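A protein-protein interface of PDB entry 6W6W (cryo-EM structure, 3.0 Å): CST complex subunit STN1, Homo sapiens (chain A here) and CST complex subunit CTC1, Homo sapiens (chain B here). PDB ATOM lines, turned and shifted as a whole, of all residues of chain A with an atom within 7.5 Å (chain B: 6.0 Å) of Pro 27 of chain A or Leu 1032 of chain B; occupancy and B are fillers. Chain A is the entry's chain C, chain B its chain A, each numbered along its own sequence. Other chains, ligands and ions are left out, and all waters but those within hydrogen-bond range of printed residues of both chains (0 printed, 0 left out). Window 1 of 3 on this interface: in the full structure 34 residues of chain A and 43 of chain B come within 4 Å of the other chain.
Of the printed residues of chain B, Leu 25 of chain A touches Asn 1207. Of chain B, only Leu 1032 (3.8 Å), Thr 1097 (3.2 Å) and Ala 1098 (3.5 Å) come within 4 Å of Pro 27 of chain A. His 58 of chain A touches none of the printed residues of chain B. Of chain A, only Pro 27 comes within 4 Å of Leu 1032 of chain B. Of the printed residues of chain A, Asn 1207 of chain B touches Leu 25 (3.95 Å). The nearest residue of chain B that does not touch Pro 27 of chain A is Ala 1029 of chain B (4.5 Å). The nearest residue of chain A that does not touch Leu 1032 of chain B is Leu 25 of chain A (6.4 Å).
The backbone carbonyl oxygen (O) of Thr 1097 of chain B sits close to the backbone carbonyl oxygen (O) of Pro 27 of chain A, 3.2 Å away. OE1 of Glu 1099 of chain B lies close to O of Leu 30 of chain A (3.3 Å).
The backbone NH (N) of Ala 1029 of chain B is in hydrogen-bond range of the side-chain hydroxyl (OG1) of Thr 1097 of chain B (3.3 Å). The side-chain carboxylate (OE2) of Glu 1099 of chain B is in salt-bridge range of the guanidinium group (NE) of Arg 1209 of chain B, at 3.3 Å.
Asn 1207 of chain B touches Leu 25 of chain A (ND2 to CD2, 3.95 Å). Pro 27 of chain A touches Leu 1032 of chain B. O of Pro 27 of chain A touches CA of Ala 1098 of chain B, at 3.5 Å. O of Thr 1097 of chain B touches N of Val 28 of chain A, at 3.5 Å. Ala 31 of chain A touches Thr 1097 of chain B (CB to C, 3.8 Å). Ala 1098 of chain B touches Ala 31 of chain A (N to CB, 3.7 Å).
Of the 13 printed residues of chain A, 5 touch a printed residue of chain B. Among the printed residues, 8 pairs touch across the chains.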
ATOM      1  N   TRP A  23     -21.308  -3.449  -9.467  1.00  0.00           N
ATOM      2  CA  TRP A  23     -20.462  -2.778  -8.489  1.00  0.00           C
ATOM      3  C   TRP A  23     -20.602  -1.268  -8.564  1.00  0.00           C
ATOM      4  O   TRP A  23     -20.601  -0.594  -7.531  1.00  0.00           O
ATOM      5  CB  TRP A  23     -19.001  -3.164  -8.693  1.00  0.00           C
ATOM      6  CG  TRP A  23     -18.639  -4.505  -8.180  1.00  0.00           C
ATOM      7  CD1 TRP A  23     -19.401  -5.317  -7.409  1.00  0.00           C
ATOM      8  CD2 TRP A  23     -17.415  -5.201  -8.410  1.00  0.00           C
ATOM      9  NE1 TRP A  23     -18.729  -6.477  -7.135  1.00  0.00           N
ATOM     10  CE2 TRP A  23     -17.504  -6.431  -7.743  1.00  0.00           C
ATOM     11  CE3 TRP A  23     -16.249  -4.900  -9.113  1.00  0.00           C
ATOM     12  CZ2 TRP A  23     -16.475  -7.360  -7.757  1.00  0.00           C
ATOM     13  CZ3 TRP A  23     -15.230  -5.823  -9.131  1.00  0.00           C
ATOM     14  CH2 TRP A  23     -15.349  -7.039  -8.457  1.00  0.00           C
ATOM     15  N   GLY A  24     -20.714  -0.719  -9.771  1.00  0.00           N
ATOM     16  CA  GLY A  24     -20.740   0.722  -9.933  1.00  0.00           C
ATOM     17  C   GLY A  24     -22.017   1.385  -9.477  1.00  0.00           C
ATOM     18  O   GLY A  24     -22.045   2.614  -9.358  1.00  0.00           O
ATOM     19  N   LEU A  25     -23.071   0.611  -9.230  1.00  0.00           N
ATOM     20  CA  LEU A  25     -24.282   1.170  -8.654  1.00  0.00           C
ATOM     21  C   LEU A  25     -24.120   1.473  -7.172  1.00  0.00           C
ATOM     22  O   LEU A  25     -24.852   2.313  -6.643  1.00  0.00           O
ATOM     23  CB  LEU A  25     -25.449   0.213  -8.874  1.00  0.00           C
ATOM     24  CG  LEU A  25     -25.675  -0.205 -10.325  1.00  0.00           C
ATOM     25  CD1 LEU A  25     -26.696  -1.315 -10.401  1.00  0.00           C
ATOM     26  CD2 LEU A  25     -26.112   0.979 -11.154  1.00  0.00           C
ATOM     27  N   ASP A  26     -23.184   0.813  -6.500  1.00  0.00           N
ATOM     28  CA  ASP A  26     -22.873   1.135  -5.113  1.00  0.00           C
ATOM     29  C   ASP A  26     -22.120   2.457  -5.052  1.00  0.00           C
ATOM     30  O   ASP A  26     -21.107   2.615  -5.741  1.00  0.00           O
ATOM     31  CB  ASP A  26     -22.030   0.028  -4.494  1.00  0.00           C
ATOM     32  CG  ASP A  26     -22.439  -0.298  -3.077  1.00  0.00           C
ATOM     33  OD1 ASP A  26     -23.098   0.536  -2.431  1.00  0.00           O
ATOM     34  OD2 ASP A  26     -22.105  -1.402  -2.607  1.00  0.00           O
ATOM     35  N   PRO A  27     -22.576   3.429  -4.256  1.00  0.00           N
ATOM     36  CA  PRO A  27     -21.863   4.711  -4.189  1.00  0.00           C
ATOM     37  C   PRO A  27     -20.528   4.642  -3.471  1.00  0.00           C
ATOM     38  O   PRO A  27     -19.722   5.565  -3.620  1.00  0.00           O
ATOM     39  CB  PRO A  27     -22.845   5.620  -3.440  1.00  0.00           C
ATOM     40  CG  PRO A  27     -24.158   4.960  -3.563  1.00  0.00           C
ATOM     41  CD  PRO A  27     -23.876   3.499  -3.576  1.00  0.00           C
ATOM     42  N   VAL A  28     -20.261   3.583  -2.701  1.00  0.00           N
ATOM     43  CA  VAL A  28     -18.985   3.451  -2.003  1.00  0.00           C
ATOM     44  C   VAL A  28     -17.887   2.941  -2.923  1.00  0.00           C
ATOM     45  O   VAL A  28     -16.712   2.930  -2.536  1.00  0.00           O
ATOM     46  CB  VAL A  28     -19.189   2.530  -0.783  1.00  0.00           C
ATOM     47  CG1 VAL A  28     -19.252   1.078  -1.206  1.00  0.00           C
ATOM     48  CG2 VAL A  28     -18.151   2.772   0.312  1.00  0.00           C
ATOM     49  N   PHE A  29     -18.234   2.536  -4.145  1.00  0.00           N
ATOM     50  CA  PHE A  29     -17.243   2.072  -5.107  1.00  0.00           C
ATOM     51  C   PHE A  29     -16.328   3.197  -5.564  1.00  0.00           C
ATOM     52  O   PHE A  29     -15.140   2.967  -5.805  1.00  0.00           O
ATOM     53  CB  PHE A  29     -17.951   1.444  -6.304  1.00  0.00           C
ATOM     54  CG  PHE A  29     -17.031   0.754  -7.265  1.00  0.00           C
ATOM     55  CD1 PHE A  29     -16.269  -0.320  -6.859  1.00  0.00           C
ATOM     56  CD2 PHE A  29     -16.946   1.175  -8.579  1.00  0.00           C
ATOM     57  CE1 PHE A  29     -15.428  -0.957  -7.742  1.00  0.00           C
ATOM     58  CE2 PHE A  29     -16.112   0.542  -9.466  1.00  0.00           C
ATOM     59  CZ  PHE A  29     -15.353  -0.525  -9.047  1.00  0.00           C
ATOM     60  N   LEU A  30     -16.848   4.415  -5.669  1.00  0.00           N
ATOM     61  CA  LEU A  30     -16.074   5.558  -6.124  1.00  0.00           C
ATOM     62  C   LEU A  30     -15.654   6.475  -4.988  1.00  0.00           C
ATOM     63  O   LEU A  30     -15.191   7.589  -5.244  1.00  0.00           O
ATOM     64  CB  LEU A  30     -16.870   6.348  -7.159  1.00  0.00           C
ATOM     65  CG  LEU A  30     -17.403   5.532  -8.329  1.00  0.00           C
ATOM     66  CD1 LEU A  30     -18.174   6.419  -9.275  1.00  0.00           C
ATOM     67  CD2 LEU A  30     -16.262   4.860  -9.045  1.00  0.00           C
ATOM     68  N   ALA A  31     -15.805   6.038  -3.746  1.00  0.00           N
ATOM     69  CA  ALA A  31     -15.440   6.829  -2.586  1.00  0.00           C
ATOM     70  C   ALA A  31     -14.248   6.208  -1.877  1.00  0.00           C
ATOM     71  O   ALA A  31     -13.984   5.010  -1.988  1.00  0.00           O
ATOM     72  CB  ALA A  31     -16.613   6.949  -1.613  1.00  0.00           C
ATOM     73  N   PHE A  32     -13.526   7.047  -1.142  1.00  0.00           N
ATOM     74  CA  PHE A  32     -12.427   6.598  -0.294  1.00  0.00           C
ATOM     75  C   PHE A  32     -13.026   6.160   1.033  1.00  0.00           C
ATOM     76  O   PHE A  32     -13.397   6.990   1.861  1.00  0.00           O
ATOM     77  CB  PHE A  32     -11.403   7.709  -0.098  1.00  0.00           C
ATOM     78  CG  PHE A  32     -10.597   8.018  -1.325  1.00  0.00           C
ATOM     79  CD1 PHE A  32     -11.092   8.862  -2.300  1.00  0.00           C
ATOM     80  CD2 PHE A  32      -9.340   7.476  -1.495  1.00  0.00           C
ATOM     81  CE1 PHE A  32     -10.353   9.146  -3.422  1.00  0.00           C
ATOM     82  CE2 PHE A  32      -8.600   7.759  -2.613  1.00  0.00           C
ATOM     83  CZ  PHE A  32      -9.105   8.595  -3.574  1.00  0.00           C
ATOM     84  N   HIS A  58     -19.925  -4.871  -0.167  1.00  0.00           N
ATOM     85  CA  HIS A  58     -19.620  -3.607  -0.820  1.00  0.00           C
ATOM     86  C   HIS A  58     -18.273  -3.704  -1.502  1.00  0.00           C
ATOM     87  O   HIS A  58     -17.303  -4.132  -0.864  1.00  0.00           O
ATOM     88  CB  HIS A  58     -19.591  -2.462   0.187  1.00  0.00           C
ATOM     89  CG  HIS A  58     -20.905  -2.191   0.843  1.00  0.00           C
ATOM     90  ND1 HIS A  58     -21.321  -2.858   1.972  1.00  0.00           N
ATOM     91  CD2 HIS A  58     -21.885  -1.309   0.544  1.00  0.00           C
ATOM     92  CE1 HIS A  58     -22.508  -2.409   2.334  1.00  0.00           C
ATOM     93  NE2 HIS A  58     -22.873  -1.468   1.484  1.00  0.00           N
ATOM     94  N   PRO A  59     -18.151  -3.332  -2.774  1.00  0.00           N
ATOM     95  CA  PRO A  59     -16.832  -3.328  -3.418  1.00  0.00           C
ATOM     96  C   PRO A  59     -16.001  -2.149  -2.934  1.00  0.00           C
ATOM     97  O   PRO A  59     -16.382  -0.991  -3.108  1.00  0.00           O
ATOM     98  CB  PRO A  59     -17.167  -3.216  -4.906  1.00  0.00           C
ATOM     99  CG  PRO A  59     -18.513  -2.600  -4.946  1.00  0.00           C
ATOM    100  CD  PRO A  59     -19.235  -3.059  -3.730  1.00  0.00           C
ATOM    101  N   PHE A 188     -26.570  -3.263   0.443  1.00  0.00           N
ATOM    102  CA  PHE A 188     -26.986  -2.482  -0.712  1.00  0.00           C
ATOM    103  C   PHE A 188     -28.046  -3.236  -1.503  1.00  0.00           C
ATOM    104  O   PHE A 188     -27.982  -4.462  -1.636  1.00  0.00           O
ATOM    105  CB  PHE A 188     -25.797  -2.157  -1.614  1.00  0.00           C
ATOM    106  CG  PHE A 188     -26.133  -1.227  -2.739  1.00  0.00           C
ATOM    107  CD1 PHE A 188     -26.383   0.112  -2.494  1.00  0.00           C
ATOM    108  CD2 PHE A 188     -26.207  -1.691  -4.039  1.00  0.00           C
ATOM    109  CE1 PHE A 188     -26.698   0.972  -3.525  1.00  0.00           C
ATOM    110  CE2 PHE A 188     -26.522  -0.838  -5.075  1.00  0.00           C
ATOM    111  CZ  PHE A 188     -26.769   0.495  -4.816  1.00  0.00           C
ATOM    112  N   LEU B1028     -23.322  12.168   1.857  1.00  0.00           N
ATOM    113  CA  LEU B1028     -23.400  12.343   0.409  1.00  0.00           C
ATOM    114  C   LEU B1028     -24.080  11.178  -0.293  1.00  0.00           C
ATOM    115  O   LEU B1028     -24.543  11.342  -1.424  1.00  0.00           O
ATOM    116  CB  LEU B1028     -22.009  12.542  -0.187  1.00  0.00           C
ATOM    117  CG  LEU B1028     -21.543  13.976  -0.438  1.00  0.00           C
ATOM    118  CD1 LEU B1028     -20.282  13.981  -1.279  1.00  0.00           C
ATOM    119  CD2 LEU B1028     -22.629  14.803  -1.091  1.00  0.00           C
ATOM    120  N   ALA B1029     -24.154  10.010   0.340  1.00  0.00           N
ATOM    121  CA  ALA B1029     -24.809   8.873  -0.288  1.00  0.00           C
ATOM    122  C   ALA B1029     -26.321   8.956  -0.209  1.00  0.00           C
ATOM    123  O   ALA B1029     -27.001   8.284  -0.988  1.00  0.00           O
ATOM    124  CB  ALA B1029     -24.350   7.566   0.350  1.00  0.00           C
ATOM    125  N   GLU B1030     -26.862   9.762   0.705  1.00  0.00           N
ATOM    126  CA  GLU B1030     -28.307   9.842   0.874  1.00  0.00           C
ATOM    127  C   GLU B1030     -28.992  10.572  -0.272  1.00  0.00           C
ATOM    128  O   GLU B1030     -30.203  10.423  -0.445  1.00  0.00           O
ATOM    129  CB  GLU B1030     -28.644  10.535   2.188  1.00  0.00           C
ATOM    130  CG  GLU B1030     -27.971   9.950   3.408  1.00  0.00           C
ATOM    131  CD  GLU B1030     -28.534  10.517   4.694  1.00  0.00           C
ATOM    132  OE1 GLU B1030     -29.605  11.151   4.642  1.00  0.00           O
ATOM    133  OE2 GLU B1030     -27.910  10.329   5.758  1.00  0.00           O
ATOM    134  N   LEU B1031     -28.251  11.361  -1.051  1.00  0.00           N
ATOM    135  CA  LEU B1031     -28.814  11.960  -2.252  1.00  0.00           C
ATOM    136  C   LEU B1031     -28.996  10.943  -3.367  1.00  0.00           C
ATOM    137  O   LEU B1031     -29.739  11.209  -4.317  1.00  0.00           O
ATOM    138  CB  LEU B1031     -27.923  13.099  -2.738  1.00  0.00           C
ATOM    139  CG  LEU B1031     -27.543  14.153  -1.703  1.00  0.00           C
ATOM    140  CD1 LEU B1031     -26.454  15.052  -2.248  1.00  0.00           C
ATOM    141  CD2 LEU B1031     -28.755  14.965  -1.315  1.00  0.00           C
ATOM    142  N   LEU B1032     -28.337   9.789  -3.276  1.00  0.00           N
ATOM    143  CA  LEU B1032     -28.416   8.747  -4.291  1.00  0.00           C
ATOM    144  C   LEU B1032     -29.401   7.650  -3.909  1.00  0.00           C
ATOM    145  O   LEU B1032     -30.317   7.338  -4.673  1.00  0.00           O
ATOM    146  CB  LEU B1032     -27.026   8.150  -4.529  1.00  0.00           C
ATOM    147  CG  LEU B1032     -25.993   9.126  -5.079  1.00  0.00           C
ATOM    148  CD1 LEU B1032     -24.616   8.509  -5.062  1.00  0.00           C
ATOM    149  CD2 LEU B1032     -26.377   9.519  -6.486  1.00  0.00           C
ATOM    150  N   GLN B1033     -29.230   7.058  -2.734  1.00  0.00           N
ATOM    151  CA  GLN B1033     -30.057   5.931  -2.333  1.00  0.00           C
ATOM    152  C   GLN B1033     -31.376   6.412  -1.738  1.00  0.00           C
ATOM    153  O   GLN B1033     -31.407   7.345  -0.930  1.00  0.00           O
ATOM    154  CB  GLN B1033     -29.285   5.023  -1.367  1.00  0.00           C
ATOM    155  CG  GLN B1033     -28.753   5.654  -0.075  1.00  0.00           C
ATOM    156  CD  GLN B1033     -29.746   5.639   1.066  1.00  0.00           C
ATOM    157  OE1 GLN B1033     -30.592   4.751   1.156  1.00  0.00           O
ATOM    158  NE2 GLN B1033     -29.647   6.624   1.948  1.00  0.00           N
ATOM    159  N   GLY B1034     -32.468   5.805  -2.188  1.00  0.00           N
ATOM    160  CA  GLY B1034     -33.781   6.090  -1.646  1.00  0.00           C
ATOM    161  C   GLY B1034     -34.346   7.418  -2.119  1.00  0.00           C
ATOM    162  O   GLY B1034     -33.735   8.171  -2.877  1.00  0.00           O
ATOM    163  N   SER B1037     -35.261  13.219  -0.179  1.00  0.00           N
ATOM    164  CA  SER B1037     -33.951  13.785   0.083  1.00  0.00           C
ATOM    165  C   SER B1037     -33.984  15.304  -0.042  1.00  0.00           C
ATOM    166  O   SER B1037     -34.752  15.846  -0.842  1.00  0.00           O
ATOM    167  CB  SER B1037     -32.911  13.221  -0.894  1.00  0.00           C
ATOM    168  OG  SER B1037     -32.916  11.806  -0.879  1.00  0.00           O
ATOM    169  N   THR B1097     -18.701   8.165   1.887  1.00  0.00           N
ATOM    170  CA  THR B1097     -19.807   7.347   1.423  1.00  0.00           C
ATOM    171  C   THR B1097     -20.064   7.426  -0.073  1.00  0.00           C
ATOM    172  O   THR B1097     -20.493   6.431  -0.653  1.00  0.00           O
ATOM    173  CB  THR B1097     -21.088   7.750   2.159  1.00  0.00           C
ATOM    174  OG1 THR B1097     -21.360   9.129   1.902  1.00  0.00           O
ATOM    175  CG2 THR B1097     -20.929   7.566   3.648  1.00  0.00           C
ATOM    176  N   ALA B1098     -19.831   8.572  -0.706  1.00  0.00           N
ATOM    177  CA  ALA B1098     -20.062   8.739  -2.135  1.00  0.00           C
ATOM    178  C   ALA B1098     -19.182   9.876  -2.633  1.00  0.00           C
ATOM    179  O   ALA B1098     -18.425  10.476  -1.869  1.00  0.00           O
ATOM    180  CB  ALA B1098     -21.537   9.011  -2.433  1.00  0.00           C
ATOM    181  N   GLU B1099     -19.288  10.171  -3.925  1.00  0.00           N
ATOM    182  CA  GLU B1099     -18.534  11.248  -4.549  1.00  0.00           C
ATOM    183  C   GLU B1099     -19.477  12.142  -5.340  1.00  0.00           C
ATOM    184  O   GLU B1099     -20.618  11.776  -5.628  1.00  0.00           O
ATOM    185  CB  GLU B1099     -17.432  10.707  -5.462  1.00  0.00           C
ATOM    186  CG  GLU B1099     -17.938  10.216  -6.795  1.00  0.00           C
ATOM    187  CD  GLU B1099     -16.824   9.967  -7.782  1.00  0.00           C
ATOM    188  OE1 GLU B1099     -15.646  10.062  -7.385  1.00  0.00           O
ATOM    189  OE2 GLU B1099     -17.126   9.688  -8.960  1.00  0.00           O
ATOM    190  N   ASN B1207     -24.648   4.848 -12.422  1.00  0.00           N
ATOM    191  CA  ASN B1207     -25.638   5.903 -12.412  1.00  0.00           C
ATOM    192  C   ASN B1207     -24.970   7.218 -12.801  1.00  0.00           C
ATOM    193  O   ASN B1207     -23.743   7.326 -12.759  1.00  0.00           O
ATOM    194  CB  ASN B1207     -26.266   5.995 -11.025  1.00  0.00           C
ATOM    195  CG  ASN B1207     -27.400   5.017 -10.841  1.00  0.00           C
ATOM    196  OD1 ASN B1207     -28.220   4.825 -11.737  1.00  0.00           O
ATOM    197  ND2 ASN B1207     -27.455   4.390  -9.673  1.00  0.00           N
ATOM    198  N   PRO B1208     -25.740   8.222 -13.229  1.00  0.00           N
ATOM    199  CA  PRO B1208     -25.140   9.535 -13.487  1.00  0.00           C
ATOM    200  C   PRO B1208     -24.627  10.185 -12.212  1.00  0.00           C
ATOM    201  O   PRO B1208     -25.180  10.005 -11.125  1.00  0.00           O
ATOM    202  CB  PRO B1208     -26.290  10.341 -14.100  1.00  0.00           C
ATOM    203  CG  PRO B1208     -27.521   9.585 -13.758  1.00  0.00           C
ATOM    204  CD  PRO B1208     -27.110   8.158 -13.763  1.00  0.00           C
ATOM    205  N   ARG B1209     -23.545  10.939 -12.362  1.00  0.00           N
ATOM    206  CA  ARG B1209     -22.810  11.467 -11.227  1.00  0.00           C
ATOM    207  C   ARG B1209     -23.543  12.656 -10.613  1.00  0.00           C
ATOM    208  O   ARG B1209     -24.264  13.386 -11.298  1.00  0.00           O
ATOM    209  CB  ARG B1209     -21.404  11.875 -11.670  1.00  0.00           C
ATOM    210  CG  ARG B1209     -20.393  12.019 -10.552  1.00  0.00           C
ATOM    211  CD  ARG B1209     -19.027  12.376 -11.094  1.00  0.00           C
ATOM    212  NE  ARG B1209     -18.302  11.228 -11.620  1.00  0.00           N
ATOM    213  CZ  ARG B1209     -17.170  11.319 -12.308  1.00  0.00           C
ATOM    214  NH1 ARG B1209     -16.639  12.505 -12.559  1.00  0.00           N
ATOM    215  NH2 ARG B1209     -16.570  10.224 -12.748  1.00  0.00           N
ATOM    216  N   LEU B1210     -23.374  12.826  -9.301  1.00  0.00           N
ATOM    217  CA  LEU B1210     -23.917  13.987  -8.609  1.00  0.00           C
ATOM    218  C   LEU B1210     -23.220  15.257  -9.065  1.00  0.00           C
ATOM    219  O   LEU B1210     -21.989  15.323  -9.099  1.00  0.00           O
ATOM    220  CB  LEU B1210     -23.758  13.840  -7.101  1.00  0.00           C
ATOM    221  CG  LEU B1210     -24.642  12.851  -6.359  1.00  0.00           C
ATOM    222  CD1 LEU B1210     -24.204  12.748  -4.918  1.00  0.00           C
ATOM    223  CD2 LEU B1210     -26.079  13.306  -6.439  1.00  0.00           C
